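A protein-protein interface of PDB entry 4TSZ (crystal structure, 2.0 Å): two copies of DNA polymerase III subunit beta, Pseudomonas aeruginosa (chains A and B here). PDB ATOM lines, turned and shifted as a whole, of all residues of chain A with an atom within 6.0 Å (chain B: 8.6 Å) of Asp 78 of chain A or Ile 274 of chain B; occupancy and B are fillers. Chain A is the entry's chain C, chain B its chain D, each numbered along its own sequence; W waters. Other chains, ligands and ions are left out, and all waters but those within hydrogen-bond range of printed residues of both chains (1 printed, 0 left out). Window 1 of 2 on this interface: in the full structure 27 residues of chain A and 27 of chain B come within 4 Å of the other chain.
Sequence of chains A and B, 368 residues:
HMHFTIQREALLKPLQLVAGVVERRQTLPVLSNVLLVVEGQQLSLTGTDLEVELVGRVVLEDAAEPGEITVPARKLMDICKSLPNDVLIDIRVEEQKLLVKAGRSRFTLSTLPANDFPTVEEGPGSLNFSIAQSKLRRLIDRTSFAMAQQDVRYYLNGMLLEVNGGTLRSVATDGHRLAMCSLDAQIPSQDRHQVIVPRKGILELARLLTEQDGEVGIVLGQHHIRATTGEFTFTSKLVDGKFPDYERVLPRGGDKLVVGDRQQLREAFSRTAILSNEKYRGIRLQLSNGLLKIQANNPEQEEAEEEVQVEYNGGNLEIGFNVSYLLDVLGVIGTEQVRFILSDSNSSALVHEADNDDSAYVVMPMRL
The backbone carbonyl oxygen of Asp 78 of chain A sits at hydrogen-bond distance from the side-chain hydroxyl of Ser 82 of chain A (3.0 Å). O of Ile 79 of chain A is in hydrogen-bond range of OG of Ser 82 of chain A (2.7 Å). The backbone NH (N) of Asn 298 of chain B sits at hydrogen-bond distance from the backbone carbonyl oxygen (O) of Leu 275 of chain B (3.3 Å). The backbone carbonyl oxygen (O) of Ala 296 of chain B sits at hydrogen-bond distance from the backbone NH (N) of Ala 304 of chain B (2.8 Å). The backbone NH (N) of Glu 300 of chain B lies within hydrogen-bond range of the side-chain amide oxygen (OD1) of Asn 298 of chain B, 3.2 Å away. OE1 of Glu 302 of chain B is in hydrogen-bond range of ND2 of Asn 298 of chain B, at 2.9 Å.
No position is printed for both chains. Of the 12 pairs that touch across the chains among the printed residues, none has its exchanged pair printed and touching as well.
NZ of Lys 75 of chain A lies within salt-bridge range of OE2 of Glu 300 of chain B, 2.6 Å away. The side-chain carboxylate of Glu 302 of chain B is in salt-bridge range of the side-chain amino group of Lys 75 of chain A, at 2.8 Å. NH1 of Arg 271 of chain B is in hydrogen-bond range of O of Ser 82 of chain A.
Of the 24 printed residues of chain B, 8 touch a printed residue of chain A. Hydrophobic or aromatic side chains of chain B within 4 Å of the printed part of chain A: Ile 274, Leu 275 and Ala 304. Of the 12 printed residues of chain A, 6 touch a printed residue of chain B. Printed residues of chain A that touch a printed residue of chain B: Lys 75, Asp 78, Ile 79, Ser 82, Leu 83 and Phe 107. Hydrophobic or aromatic side chains of chain A within 4 Å of the printed part of chain B: Ile 79, Leu 83 and Phe 107. Along chain A the printed residues that touch a printed residue of chain B span positions 75 to 107. Among the printed residues, 12 pairs touch across the chains. Among the printed residues, Asp or Glu carboxylates within 4 Å of a Lys or Arg side-chain nitrogen of the other chain: Lys 75 of chain A with Glu 300 of chain B (2.6 Å) and Lys 75 of chain A with Glu 302 of chain B (2.8 Å).
Among the printed residues, merely in contact across the chains: Phe 107 of chain A with Glu 303 of chain B, Ser 82 of chain A with Ile 274 of chain B, Asp 78 of chain A with Ile 274 of chain B, Phe 107 of chain A with Arg 271 of chain B, Phe 107 of chain A with Ala 304 of chain B, Ile 79 of chain A with Ile 274 of chain B, Leu 83 of chain A with Arg 271 of chain B, Lys 75 of chain A with Asn 298 of chain B and Phe 107 of chain A with Leu 275 of chain B.
Water W1 bridges the backbone carbonyl oxygen (O) of Ser 82 of chain A (2.9 Å) and the backbone carbonyl oxygen (O) of Glu 267 of chain B (3.0 Å).
Asp 78 of chain A touches just one residue of chain B: Ile 274. Of the printed residues of chain A, Ile 274 of chain B touches Asp 78 (3.3 Å), Ile 79 (3.8 Å) and Ser 82 (3.3 Å). Printed residues of chain A within 4 Å of Glu 302 of chain B: Lys 75 (2.8 Å). Of the printed residues of chain A, Arg 271 of chain B touches Ser 82 (2.9 Å), Leu 83 (3.8 Å) and Phe 107 (3.6 Å). Printed residues of chain A within 4 Å of Ala 304 of chain B: Phe 107 (3.8 Å). Of the printed residues of chain A, Glu 303 of chain B touches Phe 107. Of the printed residues of chain B, Lys 75 of chain A touches Asn 298, Glu 300 and Glu 302. The nearest residue of chain B that does not touch Asp 78 of chain A is Arg 271 of chain B (6.3 Å). The nearest printed residue of chain B that does not touch Lys 75 of chain A is Ile 274 of chain B (4.01 Å).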
ATOM      1  N   ALA A  73      -4.673   7.291 -21.807  1.00  0.00           N
ATOM      2  CA  ALA A  73      -4.362   7.520 -20.395  1.00  0.00           C
ATOM      3  C   ALA A  73      -3.053   6.892 -19.913  1.00  0.00           C
ATOM      4  O   ALA A  73      -2.231   7.597 -19.324  1.00  0.00           O
ATOM      5  CB  ALA A  73      -5.534   7.098 -19.518  1.00  0.00           C
ATOM      6  N   ARG A  74      -2.846   5.590 -20.184  1.00  0.00           N
ATOM      7  CA  ARG A  74      -1.632   4.859 -19.792  1.00  0.00           C
ATOM      8  C   ARG A  74      -0.383   5.452 -20.450  1.00  0.00           C
ATOM      9  O   ARG A  74       0.611   5.684 -19.760  1.00  0.00           O
ATOM     10  CB  ARG A  74      -1.776   3.344 -20.077  1.00  0.00           C
ATOM     11  CG  ARG A  74      -0.571   2.470 -19.663  1.00  0.00           C
ATOM     12  CD  ARG A  74      -0.504   2.171 -18.173  1.00  0.00           C
ATOM     13  NE  ARG A  74      -1.589   1.293 -17.730  1.00  0.00           N
ATOM     14  CZ  ARG A  74      -1.413   0.173 -17.033  1.00  0.00           C
ATOM     15  NH1 ARG A  74      -0.193  -0.216 -16.683  1.00  0.00           N
ATOM     16  NH2 ARG A  74      -2.457  -0.561 -16.675  1.00  0.00           N
ATOM     17  N   LYS A  75      -0.456   5.747 -21.763  1.00  0.00           N
ATOM     18  CA  LYS A  75       0.656   6.349 -22.498  1.00  0.00           C
ATOM     19  C   LYS A  75       1.059   7.708 -21.928  1.00  0.00           C
ATOM     20  O   LYS A  75       2.247   7.911 -21.689  1.00  0.00           O
ATOM     21  CB  LYS A  75       0.367   6.436 -24.003  1.00  0.00           C
ATOM     22  CG  LYS A  75       0.779   5.182 -24.748  1.00  0.00           C
ATOM     23  CD  LYS A  75       0.273   5.213 -26.154  1.00  0.00           C
ATOM     24  CE  LYS A  75       0.443   3.891 -26.843  1.00  0.00           C
ATOM     25  NZ  LYS A  75      -0.504   3.763 -27.981  1.00  0.00           N
ATOM     26  N   LEU A  76       0.083   8.620 -21.676  1.00  0.00           N
ATOM     27  CA  LEU A  76       0.374   9.943 -21.117  1.00  0.00           C
ATOM     28  C   LEU A  76       0.969   9.831 -19.710  1.00  0.00           C
ATOM     29  O   LEU A  76       1.927  10.544 -19.407  1.00  0.00           O
ATOM     30  CB  LEU A  76      -0.852  10.874 -21.147  1.00  0.00           C
ATOM     31  CG  LEU A  76      -0.629  12.336 -20.675  1.00  0.00           C
ATOM     32  CD1 LEU A  76       0.255  13.128 -21.645  1.00  0.00           C
ATOM     33  CD2 LEU A  76      -1.956  13.052 -20.471  1.00  0.00           C
ATOM     34  N   MET A  77       0.428   8.920 -18.875  1.00  0.00           N
ATOM     35  CA  MET A  77       0.940   8.677 -17.527  1.00  0.00           C
ATOM     36  C   MET A  77       2.389   8.157 -17.593  1.00  0.00           C
ATOM     37  O   MET A  77       3.241   8.689 -16.881  1.00  0.00           O
ATOM     38  CB  MET A  77       0.034   7.703 -16.767  1.00  0.00           C
ATOM     39  CG  MET A  77       0.391   7.575 -15.299  1.00  0.00           C
ATOM     40  SD  MET A  77      -0.375   6.109 -14.564  1.00  0.00           S
ATOM     41  N   ASP A  78       2.668   7.163 -18.476  1.00  0.00           N
ATOM     42  CA  ASP A  78       4.002   6.580 -18.653  1.00  0.00           C
ATOM     43  C   ASP A  78       5.019   7.603 -19.132  1.00  0.00           C
ATOM     44  O   ASP A  78       6.154   7.589 -18.659  1.00  0.00           O
ATOM     45  CB  ASP A  78       3.973   5.353 -19.583  1.00  0.00           C
ATOM     46  CG  ASP A  78       3.293   4.116 -19.012  1.00  0.00           C
ATOM     47  OD1 ASP A  78       3.038   4.085 -17.785  1.00  0.00           O
ATOM     48  OD2 ASP A  78       3.008   3.186 -19.794  1.00  0.00           O
ATOM     49  N   ILE A  79       4.601   8.519 -20.038  1.00  0.00           N
ATOM     50  CA  ILE A  79       5.457   9.597 -20.541  1.00  0.00           C
ATOM     51  C   ILE A  79       5.772  10.537 -19.366  1.00  0.00           C
ATOM     52  O   ILE A  79       6.943  10.812 -19.109  1.00  0.00           O
ATOM     53  CB  ILE A  79       4.806  10.315 -21.755  1.00  0.00           C
ATOM     54  CG1 ILE A  79       4.918   9.459 -23.032  1.00  0.00           C
ATOM     55  CG2 ILE A  79       5.392  11.721 -21.964  1.00  0.00           C
ATOM     56  CD1 ILE A  79       3.863   9.755 -24.081  1.00  0.00           C
ATOM     57  N   CYS A  80       4.730  10.958 -18.624  1.00  0.00           N
ATOM     58  CA  CYS A  80       4.840  11.830 -17.452  1.00  0.00           C
ATOM     59  C   CYS A  80       5.789  11.233 -16.393  1.00  0.00           C
ATOM     60  O   CYS A  80       6.732  11.912 -15.979  1.00  0.00           O
ATOM     61  CB  CYS A  80       3.458  12.144 -16.878  1.00  0.00           C
ATOM     62  SG  CYS A  80       3.428  13.555 -15.741  1.00  0.00           S
ATOM     63  N   LYS A  81       5.594   9.943 -16.026  1.00  0.00           N
ATOM     64  CA  LYS A  81       6.430   9.231 -15.052  1.00  0.00           C
ATOM     65  C   LYS A  81       7.910   9.123 -15.504  1.00  0.00           C
ATOM     66  O   LYS A  81       8.820   9.264 -14.680  1.00  0.00           O
ATOM     67  CB  LYS A  81       5.871   7.821 -14.799  1.00  0.00           C
ATOM     68  CG  LYS A  81       5.540   7.531 -13.340  1.00  0.00           C
ATOM     69  CD  LYS A  81       4.881   6.161 -13.145  1.00  0.00           C
ATOM     70  CE  LYS A  81       3.408   6.125 -13.512  1.00  0.00           C
ATOM     71  NZ  LYS A  81       2.737   4.902 -12.999  1.00  0.00           N
ATOM     72  N   SER A  82       8.139   8.890 -16.804  1.00  0.00           N
ATOM     73  CA  SER A  82       9.470   8.732 -17.396  1.00  0.00           C
ATOM     74  C   SER A  82      10.257  10.043 -17.562  1.00  0.00           C
ATOM     75  O   SER A  82      11.473  10.004 -17.761  1.00  0.00           O
ATOM     76  CB  SER A  82       9.366   8.007 -18.734  1.00  0.00           C
ATOM     77  OG  SER A  82       8.700   8.826 -19.679  1.00  0.00           O
ATOM     78  N   LEU A  83       9.571  11.195 -17.503  1.00  0.00           N
ATOM     79  CA  LEU A  83      10.217  12.499 -17.649  1.00  0.00           C
ATOM     80  C   LEU A  83      11.094  12.848 -16.440  1.00  0.00           C
ATOM     81  O   LEU A  83      10.823  12.342 -15.348  1.00  0.00           O
ATOM     82  CB  LEU A  83       9.172  13.594 -17.910  1.00  0.00           C
ATOM     83  CG  LEU A  83       8.629  13.653 -19.340  1.00  0.00           C
ATOM     84  CD1 LEU A  83       7.441  14.567 -19.425  1.00  0.00           C
ATOM     85  CD2 LEU A  83       9.705  14.068 -20.334  1.00  0.00           C
ATOM     86  N   PHE A 107       6.968  14.483 -27.753  1.00  0.00           N
ATOM     87  CA  PHE A 107       6.020  13.387 -27.934  1.00  0.00           C
ATOM     88  C   PHE A 107       4.793  13.847 -28.693  1.00  0.00           C
ATOM     89  O   PHE A 107       4.288  14.946 -28.450  1.00  0.00           O
ATOM     90  CB  PHE A 107       5.574  12.795 -26.579  1.00  0.00           C
ATOM     91  CG  PHE A 107       6.689  12.381 -25.649  1.00  0.00           C
ATOM     92  CD1 PHE A 107       7.261  13.299 -24.770  1.00  0.00           C
ATOM     93  CD2 PHE A 107       7.171  11.073 -25.650  1.00  0.00           C
ATOM     94  CE1 PHE A 107       8.305  12.921 -23.922  1.00  0.00           C
ATOM     95  CE2 PHE A 107       8.219  10.696 -24.798  1.00  0.00           C
ATOM     96  CZ  PHE A 107       8.776  11.625 -23.940  1.00  0.00           C
ATOM     97  N   GLU B 267      17.462   6.556 -19.575  1.00  0.00           N
ATOM     98  CA  GLU B 267      16.274   7.414 -19.396  1.00  0.00           C
ATOM     99  C   GLU B 267      15.651   7.833 -20.726  1.00  0.00           C
ATOM    100  O   GLU B 267      14.428   7.766 -20.869  1.00  0.00           O
ATOM    101  CB  GLU B 267      16.598   8.648 -18.540  1.00  0.00           C
ATOM    102  CG  GLU B 267      16.737   8.311 -17.068  1.00  0.00           C
ATOM    103  CD  GLU B 267      17.653   9.201 -16.256  1.00  0.00           C
ATOM    104  OE1 GLU B 267      17.887   8.853 -15.079  1.00  0.00           O
ATOM    105  OE2 GLU B 267      18.144  10.226 -16.784  1.00  0.00           O
ATOM    106  N   ALA B 268      16.500   8.245 -21.699  1.00  0.00           N
ATOM    107  CA  ALA B 268      16.067   8.636 -23.042  1.00  0.00           C
ATOM    108  C   ALA B 268      15.501   7.446 -23.810  1.00  0.00           C
ATOM    109  O   ALA B 268      14.486   7.606 -24.487  1.00  0.00           O
ATOM    110  CB  ALA B 268      17.218   9.255 -23.804  1.00  0.00           C
ATOM    111  N   PHE B 269      16.148   6.254 -23.703  1.00  0.00           N
ATOM    112  CA  PHE B 269      15.660   5.033 -24.349  1.00  0.00           C
ATOM    113  C   PHE B 269      14.325   4.610 -23.742  1.00  0.00           C
ATOM    114  O   PHE B 269      13.428   4.263 -24.491  1.00  0.00           O
ATOM    115  CB  PHE B 269      16.696   3.886 -24.299  1.00  0.00           C
ATOM    116  CG  PHE B 269      17.915   4.038 -25.188  1.00  0.00           C
ATOM    117  CD1 PHE B 269      17.829   4.683 -26.418  1.00  0.00           C
ATOM    118  CD2 PHE B 269      19.132   3.472 -24.828  1.00  0.00           C
ATOM    119  CE1 PHE B 269      18.956   4.816 -27.238  1.00  0.00           C
ATOM    120  CE2 PHE B 269      20.260   3.603 -25.650  1.00  0.00           C
ATOM    121  CZ  PHE B 269      20.164   4.274 -26.847  1.00  0.00           C
ATOM    122  N   SER B 270      14.173   4.692 -22.401  1.00  0.00           N
ATOM    123  CA  SER B 270      12.911   4.360 -21.719  1.00  0.00           C
ATOM    124  C   SER B 270      11.756   5.303 -22.133  1.00  0.00           C
ATOM    125  O   SER B 270      10.650   4.819 -22.388  1.00  0.00           O
ATOM    126  CB  SER B 270      13.076   4.396 -20.206  1.00  0.00           C
ATOM    127  OG  SER B 270      13.958   3.388 -19.753  1.00  0.00           O
ATOM    128  N   ARG B 271      12.020   6.616 -22.244  1.00  0.00           N
ATOM    129  CA  ARG B 271      11.015   7.604 -22.666  1.00  0.00           C
ATOM    130  C   ARG B 271      10.537   7.341 -24.090  1.00  0.00           C
ATOM    131  O   ARG B 271       9.330   7.258 -24.315  1.00  0.00           O
ATOM    132  CB  ARG B 271      11.547   9.045 -22.560  1.00  0.00           C
ATOM    133  CG  ARG B 271      11.600   9.573 -21.139  1.00  0.00           C
ATOM    134  CD  ARG B 271      11.904  11.056 -21.085  1.00  0.00           C
ATOM    135  NE  ARG B 271      13.328  11.342 -21.264  1.00  0.00           N
ATOM    136  CZ  ARG B 271      14.217  11.402 -20.279  1.00  0.00           C
ATOM    137  NH1 ARG B 271      13.846  11.180 -19.026  1.00  0.00           N
ATOM    138  NH2 ARG B 271      15.484  11.684 -20.540  1.00  0.00           N
ATOM    139  N   THR B 272      11.487   7.190 -25.040  1.00  0.00           N
ATOM    140  CA  THR B 272      11.174   6.932 -26.445  1.00  0.00           C
ATOM    141  C   THR B 272      10.488   5.589 -26.661  1.00  0.00           C
ATOM    142  O   THR B 272       9.586   5.514 -27.496  1.00  0.00           O
ATOM    143  CB  THR B 272      12.379   7.166 -27.375  1.00  0.00           C
ATOM    144  OG1 THR B 272      13.445   6.295 -27.004  1.00  0.00           O
ATOM    145  CG2 THR B 272      12.853   8.606 -27.369  1.00  0.00           C
ATOM    146  N   ALA B 273      10.874   4.553 -25.870  1.00  0.00           N
ATOM    147  CA  ALA B 273      10.314   3.197 -25.921  1.00  0.00           C
ATOM    148  C   ALA B 273       8.787   3.166 -25.776  1.00  0.00           C
ATOM    149  O   ALA B 273       8.147   2.337 -26.416  1.00  0.00           O
ATOM    150  CB  ALA B 273      10.958   2.315 -24.863  1.00  0.00           C
ATOM    151  N   ILE B 274       8.211   4.088 -24.969  1.00  0.00           N
ATOM    152  CA  ILE B 274       6.760   4.222 -24.749  1.00  0.00           C
ATOM    153  C   ILE B 274       6.007   4.345 -26.091  1.00  0.00           C
ATOM    154  O   ILE B 274       4.938   3.747 -26.263  1.00  0.00           O
ATOM    155  CB  ILE B 274       6.440   5.394 -23.780  1.00  0.00           C
ATOM    156  CG1 ILE B 274       7.078   5.143 -22.390  1.00  0.00           C
ATOM    157  CG2 ILE B 274       4.905   5.652 -23.663  1.00  0.00           C
ATOM    158  CD1 ILE B 274       7.343   6.428 -21.566  1.00  0.00           C
ATOM    159  N   LEU B 275       6.587   5.095 -27.038  1.00  0.00           N
ATOM    160  CA  LEU B 275       5.974   5.287 -28.354  1.00  0.00           C
ATOM    161  C   LEU B 275       6.547   4.431 -29.481  1.00  0.00           C
ATOM    162  O   LEU B 275       6.243   4.660 -30.648  1.00  0.00           O
ATOM    163  CB  LEU B 275       5.819   6.777 -28.711  1.00  0.00           C
ATOM    164  CG  LEU B 275       5.021   7.617 -27.688  1.00  0.00           C
ATOM    165  CD1 LEU B 275       4.874   9.039 -28.162  1.00  0.00           C
ATOM    166  CD2 LEU B 275       3.650   6.996 -27.386  1.00  0.00           C
ATOM    167  N   SER B 276       7.331   3.402 -29.128  1.00  0.00           N
ATOM    168  CA  SER B 276       7.826   2.448 -30.115  1.00  0.00           C
ATOM    169  C   SER B 276       6.746   1.340 -30.275  1.00  0.00           C
ATOM    170  O   SER B 276       5.879   1.193 -29.405  1.00  0.00           O
ATOM    171  CB  SER B 276       9.154   1.836 -29.664  1.00  0.00           C
ATOM    172  OG  SER B 276       9.012   0.920 -28.587  1.00  0.00           O
ATOM    173  N   ASN B 277       6.806   0.582 -31.374  1.00  0.00           N
ATOM    174  CA  ASN B 277       5.908  -0.546 -31.646  1.00  0.00           C
ATOM    175  C   ASN B 277       5.979  -1.513 -30.440  1.00  0.00           C
ATOM    176  O   ASN B 277       7.080  -1.865 -30.002  1.00  0.00           O
ATOM    177  CB  ASN B 277       6.343  -1.249 -32.930  1.00  0.00           C
ATOM    178  CG  ASN B 277       5.390  -2.313 -33.422  1.00  0.00           C
ATOM    179  OD1 ASN B 277       5.179  -3.351 -32.791  1.00  0.00           O
ATOM    180  ND2 ASN B 277       4.843  -2.080 -34.583  1.00  0.00           N
ATOM    181  N   GLU B 278       4.817  -1.879 -29.868  1.00  0.00           N
ATOM    182  CA  GLU B 278       4.760  -2.736 -28.675  1.00  0.00           C
ATOM    183  C   GLU B 278       5.370  -4.124 -28.875  1.00  0.00           C
ATOM    184  O   GLU B 278       5.911  -4.698 -27.939  1.00  0.00           O
ATOM    185  CB  GLU B 278       3.328  -2.816 -28.105  1.00  0.00           C
ATOM    186  N   ARG B 281       9.419  -3.029 -31.116  1.00  0.00           N
ATOM    187  CA  ARG B 281      10.237  -2.166 -30.259  1.00  0.00           C
ATOM    188  C   ARG B 281      11.368  -1.385 -30.958  1.00  0.00           C
ATOM    189  O   ARG B 281      12.390  -1.074 -30.342  1.00  0.00           O
ATOM    190  CB  ARG B 281      10.749  -3.022 -29.079  1.00  0.00           C
ATOM    191  CG  ARG B 281       9.618  -3.645 -28.233  1.00  0.00           C
ATOM    192  CD  ARG B 281       9.014  -2.664 -27.243  1.00  0.00           C
ATOM    193  NE  ARG B 281       9.964  -2.384 -26.180  1.00  0.00           N
ATOM    194  CZ  ARG B 281       9.814  -1.451 -25.253  1.00  0.00           C
ATOM    195  NH1 ARG B 281       8.752  -0.654 -25.266  1.00  0.00           N
ATOM    196  NH2 ARG B 281      10.732  -1.293 -24.311  1.00  0.00           N
ATOM    197  N   GLY B 282      11.157  -1.069 -32.236  1.00  0.00           N
ATOM    198  CA  GLY B 282      12.129  -0.363 -33.058  1.00  0.00           C
ATOM    199  C   GLY B 282      12.258   1.115 -32.777  1.00  0.00           C
ATOM    200  O   GLY B 282      11.254   1.821 -32.641  1.00  0.00           O
ATOM    201  N   ILE B 283      13.511   1.576 -32.661  1.00  0.00           N
ATOM    202  CA  ILE B 283      13.880   2.976 -32.486  1.00  0.00           C
ATOM    203  C   ILE B 283      14.918   3.324 -33.538  1.00  0.00           C
ATOM    204  O   ILE B 283      15.625   2.433 -34.012  1.00  0.00           O
ATOM    205  CB  ILE B 283      14.339   3.364 -31.047  1.00  0.00           C
ATOM    206  CG1 ILE B 283      15.608   2.603 -30.605  1.00  0.00           C
ATOM    207  CG2 ILE B 283      13.185   3.253 -30.048  1.00  0.00           C
ATOM    208  CD1 ILE B 283      16.373   3.226 -29.488  1.00  0.00           C
ATOM    209  N   ALA B 296      11.271   7.282 -32.115  1.00  0.00           N
ATOM    210  CA  ALA B 296      10.420   6.105 -32.047  1.00  0.00           C
ATOM    211  C   ALA B 296       9.027   6.435 -32.517  1.00  0.00           C
ATOM    212  O   ALA B 296       8.496   7.498 -32.195  1.00  0.00           O
ATOM    213  CB  ALA B 296      10.377   5.560 -30.629  1.00  0.00           C
ATOM    214  N   ASN B 297       8.435   5.527 -33.293  1.00  0.00           N
ATOM    215  CA  ASN B 297       7.057   5.651 -33.754  1.00  0.00           C
ATOM    216  C   ASN B 297       6.342   4.302 -33.760  1.00  0.00           C
ATOM    217  O   ASN B 297       6.994   3.254 -33.721  1.00  0.00           O
ATOM    218  CB  ASN B 297       6.903   6.451 -35.051  1.00  0.00           C
ATOM    219  CG  ASN B 297       7.731   5.959 -36.193  1.00  0.00           C
ATOM    220  OD1 ASN B 297       7.502   4.869 -36.737  1.00  0.00           O
ATOM    221  ND2 ASN B 297       8.695   6.771 -36.594  1.00  0.00           N
ATOM    222  N   ASN B 298       5.007   4.336 -33.688  1.00  0.00           N
ATOM    223  CA  ASN B 298       4.196   3.131 -33.594  1.00  0.00           C
ATOM    224  C   ASN B 298       3.134   3.076 -34.721  1.00  0.00           C
ATOM    225  O   ASN B 298       3.036   4.052 -35.484  1.00  0.00           O
ATOM    226  CB  ASN B 298       3.600   3.029 -32.164  1.00  0.00           C
ATOM    227  CG  ASN B 298       2.618   4.112 -31.765  1.00  0.00           C
ATOM    228  OD1 ASN B 298       2.013   4.780 -32.598  1.00  0.00           O
ATOM    229  ND2 ASN B 298       2.384   4.252 -30.468  1.00  0.00           N
ATOM    230  N   GLU B 300      -0.045   3.579 -34.694  1.00  0.00           N
ATOM    231  CA  GLU B 300      -1.034   4.656 -34.489  1.00  0.00           C
ATOM    232  C   GLU B 300      -0.473   6.034 -34.901  1.00  0.00           C
ATOM    233  O   GLU B 300      -1.150   7.051 -34.727  1.00  0.00           O
ATOM    234  CB  GLU B 300      -1.515   4.711 -33.026  1.00  0.00           C
ATOM    235  CG  GLU B 300      -2.092   3.415 -32.483  1.00  0.00           C
ATOM    236  CD  GLU B 300      -1.176   2.724 -31.490  1.00  0.00           C
ATOM    237  OE1 GLU B 300      -0.291   1.950 -31.921  1.00  0.00           O
ATOM    238  OE2 GLU B 300      -1.341   2.969 -30.274  1.00  0.00           O
ATOM    239  N   GLU B 302       1.972   7.685 -33.521  1.00  0.00           N
ATOM    240  CA  GLU B 302       2.445   8.416 -32.348  1.00  0.00           C
ATOM    241  C   GLU B 302       3.964   8.441 -32.422  1.00  0.00           C
ATOM    242  O   GLU B 302       4.559   7.469 -32.883  1.00  0.00           O
ATOM    243  CB  GLU B 302       1.969   7.750 -31.059  1.00  0.00           C
ATOM    244  CG  GLU B 302       0.463   7.825 -30.902  1.00  0.00           C
ATOM    245  CD  GLU B 302      -0.104   7.096 -29.711  1.00  0.00           C
ATOM    246  OE1 GLU B 302       0.411   6.008 -29.373  1.00  0.00           O
ATOM    247  OE2 GLU B 302      -1.108   7.591 -29.152  1.00  0.00           O
ATOM    248  N   GLU B 303       4.594   9.550 -32.024  1.00  0.00           N
ATOM    249  CA  GLU B 303       6.040   9.683 -32.150  1.00  0.00           C
ATOM    250  C   GLU B 303       6.729  10.306 -30.936  1.00  0.00           C
ATOM    251  O   GLU B 303       6.226  11.266 -30.366  1.00  0.00           O
ATOM    252  CB  GLU B 303       6.363  10.488 -33.421  1.00  0.00           C
ATOM    253  CG  GLU B 303       7.813  10.432 -33.853  1.00  0.00           C
ATOM    254  CD  GLU B 303       8.053  11.070 -35.203  1.00  0.00           C
ATOM    255  OE1 GLU B 303       8.217  12.310 -35.255  1.00  0.00           O
ATOM    256  OE2 GLU B 303       8.037  10.332 -36.215  1.00  0.00           O
ATOM    257  N   ALA B 304       7.896   9.747 -30.564  1.00  0.00           N
ATOM    258  CA  ALA B 304       8.748  10.221 -29.474  1.00  0.00           C
ATOM    259  C   ALA B 304      10.119  10.578 -30.032  1.00  0.00           C
ATOM    260  O   ALA B 304      10.650   9.862 -30.885  1.00  0.00           O
ATOM    261  CB  ALA B 304       8.880   9.166 -28.396  1.00  0.00           C
ATOM    262  N   VAL B 323      14.817  -1.294 -28.915  1.00  0.00           N
ATOM    263  CA  VAL B 323      15.051  -0.522 -27.691  1.00  0.00           C
ATOM    264  C   VAL B 323      15.163  -1.390 -26.424  1.00  0.00           C
ATOM    265  O   VAL B 323      15.973  -1.079 -25.552  1.00  0.00           O
ATOM    266  CB  VAL B 323      14.105   0.704 -27.558  1.00  0.00           C
ATOM    267  CG1 VAL B 323      12.668   0.281 -27.299  1.00  0.00           C
ATOM    268  CG2 VAL B 323      14.585   1.678 -26.488  1.00  0.00           C
ATOM    269  N   LEU B 327      18.138  -1.468 -23.717  1.00  0.00           N
ATOM    270  CA  LEU B 327      17.813  -1.301 -22.294  1.00  0.00           C
ATOM    271  C   LEU B 327      18.326  -2.472 -21.470  1.00  0.00           C
ATOM    272  O   LEU B 327      18.854  -2.255 -20.375  1.00  0.00           O
ATOM    273  CB  LEU B 327      16.313  -1.029 -22.057  1.00  0.00           C
ATOM    274  CG  LEU B 327      15.822   0.359 -22.477  1.00  0.00           C
ATOM    275  CD1 LEU B 327      14.333   0.363 -22.736  1.00  0.00           C
ATOM    276  CD2 LEU B 327      16.199   1.413 -21.447  1.00  0.00           C
HETATM  277  O   HOH W   1      12.915   7.488 -18.237  1.00  0.00           O
